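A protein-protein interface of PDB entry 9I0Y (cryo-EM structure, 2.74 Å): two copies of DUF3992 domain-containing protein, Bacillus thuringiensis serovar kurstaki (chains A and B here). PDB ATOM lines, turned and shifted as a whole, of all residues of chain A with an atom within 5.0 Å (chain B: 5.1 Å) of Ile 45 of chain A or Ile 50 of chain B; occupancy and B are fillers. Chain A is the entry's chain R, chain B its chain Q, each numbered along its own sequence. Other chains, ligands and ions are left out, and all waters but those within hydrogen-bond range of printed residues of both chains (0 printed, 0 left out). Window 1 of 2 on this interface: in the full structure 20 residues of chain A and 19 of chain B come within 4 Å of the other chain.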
ATOM      1  N   ASN A  43      23.806  12.537 -36.268  1.00  0.00           N
ATOM      2  CA  ASN A  43      23.496  12.245 -34.876  1.00  0.00           C
ATOM      3  C   ASN A  43      23.439  10.737 -34.682  1.00  0.00           C
ATOM      4  O   ASN A  43      23.360   9.968 -35.644  1.00  0.00           O
ATOM      5  CB  ASN A  43      22.178  12.901 -34.443  1.00  0.00           C
ATOM      6  CG  ASN A  43      20.961  12.192 -35.002  1.00  0.00           C
ATOM      7  OD1 ASN A  43      20.426  11.273 -34.386  1.00  0.00           O
ATOM      8  ND2 ASN A  43      20.509  12.624 -36.170  1.00  0.00           N
ATOM      9  N   ASN A  44      23.486  10.318 -33.416  1.00  0.00           N
ATOM     10  CA  ASN A  44      23.392   8.910 -33.045  1.00  0.00           C
ATOM     11  C   ASN A  44      22.186   8.638 -32.153  1.00  0.00           C
ATOM     12  O   ASN A  44      22.157   7.638 -31.431  1.00  0.00           O
ATOM     13  CB  ASN A  44      24.678   8.443 -32.363  1.00  0.00           C
ATOM     14  CG  ASN A  44      24.854   9.036 -30.980  1.00  0.00           C
ATOM     15  OD1 ASN A  44      24.365  10.126 -30.693  1.00  0.00           O
ATOM     16  ND2 ASN A  44      25.553   8.316 -30.113  1.00  0.00           N
ATOM     17  N   ILE A  45      21.186   9.515 -32.192  1.00  0.00           N
ATOM     18  CA  ILE A  45      20.012   9.420 -31.331  1.00  0.00           C
ATOM     19  C   ILE A  45      18.751   9.337 -32.187  1.00  0.00           C
ATOM     20  O   ILE A  45      17.698   9.871 -31.820  1.00  0.00           O
ATOM     21  CB  ILE A  45      19.973  10.589 -30.328  1.00  0.00           C
ATOM     22  CG1 ILE A  45      19.712  11.924 -31.021  1.00  0.00           C
ATOM     23  CG2 ILE A  45      21.284  10.675 -29.578  1.00  0.00           C
ATOM     24  CD1 ILE A  45      20.138  13.111 -30.191  1.00  0.00           C
ATOM     25  N   ASN A  46      18.860   8.650 -33.328  1.00  0.00           N
ATOM     26  CA  ASN A  46      17.798   8.639 -34.333  1.00  0.00           C
ATOM     27  C   ASN A  46      16.450   8.236 -33.745  1.00  0.00           C
ATOM     28  O   ASN A  46      15.402   8.710 -34.199  1.00  0.00           O
ATOM     29  CB  ASN A  46      18.178   7.697 -35.472  1.00  0.00           C
ATOM     30  CG  ASN A  46      19.671   7.585 -35.651  1.00  0.00           C
ATOM     31  OD1 ASN A  46      20.371   8.590 -35.747  1.00  0.00           O
ATOM     32  ND2 ASN A  46      20.170   6.358 -35.701  1.00  0.00           N
ATOM     33  N   GLN A  47      16.448   7.354 -32.752  1.00  0.00           N
ATOM     34  CA  GLN A  47      15.197   6.979 -32.107  1.00  0.00           C
ATOM     35  C   GLN A  47      14.647   8.166 -31.324  1.00  0.00           C
ATOM     36  O   GLN A  47      15.346   8.738 -30.481  1.00  0.00           O
ATOM     37  CB  GLN A  47      15.412   5.781 -31.187  1.00  0.00           C
ATOM     38  CG  GLN A  47      14.126   5.146 -30.687  1.00  0.00           C
ATOM     39  CD  GLN A  47      14.289   4.474 -29.340  1.00  0.00           C
ATOM     40  OE1 GLN A  47      15.402   4.190 -28.905  1.00  0.00           O
ATOM     41  NE2 GLN A  47      13.174   4.216 -28.671  1.00  0.00           N
ATOM     42  N   ASN A  48      13.397   8.532 -31.607  1.00  0.00           N
ATOM     43  CA  ASN A  48      12.744   9.682 -30.987  1.00  0.00           C
ATOM     44  C   ASN A  48      13.534  10.968 -31.197  1.00  0.00           C
ATOM     45  O   ASN A  48      13.922  11.630 -30.234  1.00  0.00           O
ATOM     46  CB  ASN A  48      12.520   9.443 -29.491  1.00  0.00           C
ATOM     47  CG  ASN A  48      11.981   8.061 -29.195  1.00  0.00           C
ATOM     48  OD1 ASN A  48      12.382   7.422 -28.224  1.00  0.00           O
ATOM     49  ND2 ASN A  48      11.053   7.598 -30.024  1.00  0.00           N
ATOM     50  N   MET A  49      13.778  11.327 -32.453  1.00  0.00           N
ATOM     51  CA  MET A  49      14.404  12.605 -32.786  1.00  0.00           C
ATOM     52  C   MET A  49      13.601  13.291 -33.877  1.00  0.00           C
ATOM     53  O   MET A  49      13.206  12.644 -34.850  1.00  0.00           O
ATOM     54  CB  MET A  49      15.853  12.412 -33.221  1.00  0.00           C
ATOM     55  CG  MET A  49      16.319  13.436 -34.248  1.00  0.00           C
ATOM     56  SD  MET A  49      16.794  15.054 -33.620  1.00  0.00           S
ATOM     57  CE  MET A  49      17.794  14.622 -32.218  1.00  0.00           C
ATOM     58  N   TYR A 119      14.517  16.091 -28.798  1.00  0.00           N
ATOM     59  CA  TYR A 119      14.860  14.725 -28.428  1.00  0.00           C
ATOM     60  C   TYR A 119      14.633  14.562 -26.931  1.00  0.00           C
ATOM     61  O   TYR A 119      14.650  15.548 -26.189  1.00  0.00           O
ATOM     62  CB  TYR A 119      16.317  14.401 -28.792  1.00  0.00           C
ATOM     63  CG  TYR A 119      17.311  15.373 -28.204  1.00  0.00           C
ATOM     64  CD1 TYR A 119      17.720  16.489 -28.917  1.00  0.00           C
ATOM     65  CD2 TYR A 119      17.825  15.185 -26.931  1.00  0.00           C
ATOM     66  CE1 TYR A 119      18.617  17.381 -28.383  1.00  0.00           C
ATOM     67  CE2 TYR A 119      18.718  16.076 -26.388  1.00  0.00           C
ATOM     68  CZ  TYR A 119      19.114  17.169 -27.117  1.00  0.00           C
ATOM     69  OH  TYR A 119      20.012  18.055 -26.576  1.00  0.00           O
ATOM     70  N   LEU A 121      15.550  13.863 -23.140  1.00  0.00           N
ATOM     71  CA  LEU A 121      16.722  13.968 -22.274  1.00  0.00           C
ATOM     72  C   LEU A 121      16.622  12.969 -21.123  1.00  0.00           C
ATOM     73  O   LEU A 121      16.911  13.273 -19.967  1.00  0.00           O
ATOM     74  CB  LEU A 121      16.855  15.394 -21.754  1.00  0.00           C
ATOM     75  CG  LEU A 121      18.254  15.890 -21.415  1.00  0.00           C
ATOM     76  CD1 LEU A 121      19.147  15.759 -22.622  1.00  0.00           C
ATOM     77  CD2 LEU A 121      18.182  17.334 -20.965  1.00  0.00           C
ATOM     78  N   ASN B  48      24.307   9.714 -19.206  1.00  0.00           N
ATOM     79  CA  ASN B  48      23.326  10.792 -19.284  1.00  0.00           C
ATOM     80  C   ASN B  48      23.971  12.122 -19.658  1.00  0.00           C
ATOM     81  O   ASN B  48      23.864  13.102 -18.918  1.00  0.00           O
ATOM     82  CB  ASN B  48      22.563  10.935 -17.962  1.00  0.00           C
ATOM     83  CG  ASN B  48      22.126   9.602 -17.397  1.00  0.00           C
ATOM     84  OD1 ASN B  48      22.188   9.379 -16.188  1.00  0.00           O
ATOM     85  ND2 ASN B  48      21.663   8.712 -18.267  1.00  0.00           N
ATOM     86  N   MET B  49      24.643  12.165 -20.804  1.00  0.00           N
ATOM     87  CA  MET B  49      25.187  13.410 -21.337  1.00  0.00           C
ATOM     88  C   MET B  49      24.800  13.545 -22.799  1.00  0.00           C
ATOM     89  O   MET B  49      24.904  12.575 -23.555  1.00  0.00           O
ATOM     90  CB  MET B  49      26.704  13.465 -21.171  1.00  0.00           C
ATOM     91  CG  MET B  49      27.405  14.244 -22.276  1.00  0.00           C
ATOM     92  SD  MET B  49      27.392  16.038 -22.138  1.00  0.00           S
ATOM     93  CE  MET B  49      27.806  16.275 -20.427  1.00  0.00           C
ATOM     94  N   ILE B  50      24.357  14.734 -23.203  1.00  0.00           N
ATOM     95  CA  ILE B  50      24.084  15.003 -24.609  1.00  0.00           C
ATOM     96  C   ILE B  50      24.747  16.318 -24.996  1.00  0.00           C
ATOM     97  O   ILE B  50      24.765  17.270 -24.211  1.00  0.00           O
ATOM     98  CB  ILE B  50      22.573  15.009 -24.914  1.00  0.00           C
ATOM     99  CG1 ILE B  50      22.341  14.769 -26.404  1.00  0.00           C
ATOM    100  CG2 ILE B  50      21.930  16.311 -24.490  1.00  0.00           C
ATOM    101  CD1 ILE B  50      21.144  13.911 -26.704  1.00  0.00           C
ATOM    102  N   GLY B  51      25.341  16.347 -26.181  1.00  0.00           N
ATOM    103  CA  GLY B  51      26.011  17.535 -26.664  1.00  0.00           C
ATOM    104  C   GLY B  51      25.658  17.879 -28.094  1.00  0.00           C
ATOM    105  O   GLY B  51      25.730  17.024 -28.979  1.00  0.00           O
ATOM    106  N   THR B  52      25.282  19.132 -28.330  1.00  0.00           N
ATOM    107  CA  THR B  52      24.965  19.632 -29.660  1.00  0.00           C
ATOM    108  C   THR B  52      25.933  20.747 -30.017  1.00  0.00           C
ATOM    109  O   THR B  52      26.222  21.616 -29.193  1.00  0.00           O
ATOM    110  CB  THR B  52      23.522  20.153 -29.728  1.00  0.00           C
ATOM    111  OG1 THR B  52      22.616  19.126 -29.311  1.00  0.00           O
ATOM    112  CG2 THR B  52      23.171  20.597 -31.140  1.00  0.00           C
ATOM    113  N   THR B  90      24.854  16.210 -32.990  1.00  0.00           N
ATOM    114  CA  THR B  90      24.171  16.046 -31.710  1.00  0.00           C
ATOM    115  C   THR B  90      24.415  14.614 -31.258  1.00  0.00           C
ATOM    116  O   THR B  90      23.938  13.675 -31.899  1.00  0.00           O
ATOM    117  CB  THR B  90      22.675  16.329 -31.832  1.00  0.00           C
ATOM    118  OG1 THR B  90      22.477  17.696 -32.205  1.00  0.00           O
ATOM    119  CG2 THR B  90      21.987  16.085 -30.506  1.00  0.00           C
ATOM    120  N   TYR B  91      25.145  14.444 -30.159  1.00  0.00           N
ATOM    121  CA  TYR B  91      25.619  13.135 -29.728  1.00  0.00           C
ATOM    122  C   TYR B  91      25.233  12.879 -28.280  1.00  0.00           C
ATOM    123  O   TYR B  91      25.059  13.812 -27.497  1.00  0.00           O
ATOM    124  CB  TYR B  91      27.138  13.032 -29.877  1.00  0.00           C
ATOM    125  CG  TYR B  91      27.593  12.927 -31.307  1.00  0.00           C
ATOM    126  CD1 TYR B  91      26.996  12.032 -32.182  1.00  0.00           C
ATOM    127  CD2 TYR B  91      28.598  13.746 -31.793  1.00  0.00           C
ATOM    128  CE1 TYR B  91      27.406  11.941 -33.494  1.00  0.00           C
ATOM    129  CE2 TYR B  91      29.005  13.666 -33.101  1.00  0.00           C
ATOM    130  CZ  TYR B  91      28.412  12.763 -33.946  1.00  0.00           C
ATOM    131  OH  TYR B  91      28.831  12.690 -35.251  1.00  0.00           O
ATOM    132  N   ARG B  92      25.107  11.603 -27.925  1.00  0.00           N
ATOM    133  CA  ARG B  92      24.845  11.207 -26.550  1.00  0.00           C
ATOM    134  C   ARG B  92      25.779  10.072 -26.151  1.00  0.00           C
ATOM    135  O   ARG B  92      26.211   9.276 -26.990  1.00  0.00           O
ATOM    136  CB  ARG B  92      23.381  10.780 -26.350  1.00  0.00           C
ATOM    137  CG  ARG B  92      23.136   9.286 -26.450  1.00  0.00           C
ATOM    138  CD  ARG B  92      21.657   8.968 -26.554  1.00  0.00           C
ATOM    139  NE  ARG B  92      20.987   9.021 -25.262  1.00  0.00           N
ATOM    140  CZ  ARG B  92      20.207   8.061 -24.784  1.00  0.00           C
ATOM    141  NH1 ARG B  92      19.978   6.953 -25.469  1.00  0.00           N
ATOM    142  NH2 ARG B  92      19.642   8.217 -23.590  1.00  0.00           N
ATOM    143  N   PHE B  94      29.022   9.954 -24.965  1.00  0.00           N
ATOM    144  CA  PHE B  94      30.340  10.026 -25.573  1.00  0.00           C
ATOM    145  C   PHE B  94      31.330  10.564 -24.552  1.00  0.00           C
ATOM    146  O   PHE B  94      30.970  11.328 -23.654  1.00  0.00           O
ATOM    147  CB  PHE B  94      30.338  10.909 -26.831  1.00  0.00           C
ATOM    148  CG  PHE B  94      29.982  12.346 -26.565  1.00  0.00           C
ATOM    149  CD1 PHE B  94      28.664  12.724 -26.369  1.00  0.00           C
ATOM    150  CD2 PHE B  94      30.962  13.318 -26.514  1.00  0.00           C
ATOM    151  CE1 PHE B  94      28.336  14.040 -26.123  1.00  0.00           C
ATOM    152  CE2 PHE B  94      30.638  14.634 -26.268  1.00  0.00           C
ATOM    153  CZ  PHE B  94      29.323  14.995 -26.073  1.00  0.00           C
ATOM    154  N   THR B 116      27.361  22.782 -26.818  1.00  0.00           N
ATOM    155  CA  THR B 116      26.499  23.017 -25.668  1.00  0.00           C
ATOM    156  C   THR B 116      26.031  21.657 -25.171  1.00  0.00           C
ATOM    157  O   THR B 116      25.552  20.834 -25.958  1.00  0.00           O
ATOM    158  CB  THR B 116      25.320  23.937 -26.017  1.00  0.00           C
ATOM    159  OG1 THR B 116      24.406  23.994 -24.917  1.00  0.00           O
ATOM    160  CG2 THR B 116      24.588  23.466 -27.261  1.00  0.00           C
ATOM    161  N   THR B 117      26.194  21.419 -23.876  1.00  0.00           N
ATOM    162  CA  THR B 117      26.006  20.103 -23.284  1.00  0.00           C
ATOM    163  C   THR B 117      24.961  20.148 -22.180  1.00  0.00           C
ATOM    164  O   THR B 117      24.953  21.064 -21.353  1.00  0.00           O
ATOM    165  CB  THR B 117      27.322  19.562 -22.715  1.00  0.00           C
ATOM    166  OG1 THR B 117      27.934  20.559 -21.891  1.00  0.00           O
ATOM    167  CG2 THR B 117      28.272  19.192 -23.837  1.00  0.00           C
ATOM    168  N   ARG B 118      24.089  19.146 -22.175  1.00  0.00           N
ATOM    169  CA  ARG B 118      23.090  18.946 -21.138  1.00  0.00           C
ATOM    170  C   ARG B 118      23.416  17.682 -20.354  1.00  0.00           C
ATOM    171  O   ARG B 118      23.769  16.644 -20.935  1.00  0.00           O
ATOM    172  CB  ARG B 118      21.683  18.842 -21.731  1.00  0.00           C
ATOM    173  CG  ARG B 118      21.463  19.709 -22.950  1.00  0.00           C
ATOM    174  CD  ARG B 118      20.012  19.696 -23.382  1.00  0.00           C
ATOM    175  NE  ARG B 118      19.225  20.703 -22.682  1.00  0.00           N
ATOM    176  CZ  ARG B 118      18.502  21.637 -23.285  1.00  0.00           C
ATOM    177  NH1 ARG B 118      18.449  21.725 -24.602  1.00  0.00           N
ATOM    178  NH2 ARG B 118      17.818  22.505 -22.546  1.00  0.00           N
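Printed residues of chain B within 4 Å of Asn 44 of chain A: Thr 90, Tyr 91 and Arg 92. Ile 45 of chain A touches just these residues of chain B: Ile 50, Thr 90 and Arg 92. Printed residues of chain B within 4 Å of Tyr 119 of chain A: Ile 50, Thr 52 and Arg 118. Of chain A, only Ile 45 (3.7 Å), Tyr 119 (3.3 Å) and Leu 121 (3.4 Å) come within 4 Å of Ile 50 of chain B. Printed residues of chain A within 4 Å of Thr 52 of chain B: Tyr 119 (3.9 Å). Of the printed residues of chain A, Thr 90 of chain B touches Asn 43, Asn 44 and Ile 45. Printed residues of chain A within 4 Å of Arg 92 of chain B: Asn 44 and Ile 45. The nearest printed residue of chain A that does not touch Arg 118 of chain B is Ile 45 of chain A (9.5 Å).
Among the printed residues, merely in contact across the chains: Asn 43 of chain A with Thr 90 of chain B, Tyr 119 of chain A with Ile 50 of chain B, Leu 121 of chain A with Ile 50 of chain B, Asn 44 of chain A with Tyr 91 of chain B, Ile 45 of chain A with Arg 92 of chain B, Ile 45 of chain A with Thr 90 of chain B, Tyr 119 of chain A with Arg 118 of chain B, Asn 44 of chain A with Thr 90 of chain B, Ile 45 of chain A with Ile 50 of chain B, Leu 121 of chain A with Arg 118 of chain B and Tyr 119 of chain A with Thr 52 of chain B.
Of the 12 printed residues of chain B, 6 touch a printed residue of chain A. Hydrophobic or aromatic side chains of chain B within 4 Å of the printed part of chain A: Ile 50 and Tyr 91. Hydrophobic or aromatic side chains of chain A within 4 Å of the printed part of chain B: Ile 45, Tyr 119 and Leu 121. Along chain A the printed residues that touch a printed residue of chain B span positions 43 to 121. Among the printed residues, no Asp or Glu carboxylate lies within 4 Å of a Lys or Arg side-chain nitrogen of the other chain.
Positions printed for both chains: 48 and 49. Of the 12 pairs that touch across the chains among the printed residues, none has its exchanged pair printed and touching as well.
The side-chain amide oxygen of Asn 46 of chain A sits close to the side-chain amide oxygen of Asn 43 of chain A, at 3.0 Å. The side-chain amide oxygen of Asn 43 of chain A is in hydrogen-bond range of the backbone NH of Ile 45 of chain A (2.9 Å). The backbone carbonyl oxygen of Ile 50 of chain B sits at hydrogen-bond distance from the backbone NH of Arg 118 of chain B, at 2.8 Å. N of Gly 51 of chain B sits at hydrogen-bond distance from O of Tyr 91 of chain B (2.9 Å). The side-chain hydroxyl (OG1) of Thr 52 of chain B sits close to the side-chain hydroxyl (OG1) of Thr 90 of chain B. The backbone NH (N) of Thr 116 of chain B sits at hydrogen-bond distance from the backbone carbonyl oxygen (O) of Thr 52 of chain B (2.9 Å).
N of Arg 92 of chain B lies within hydrogen-bond range of OD1 of Asn 44 of chain A.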
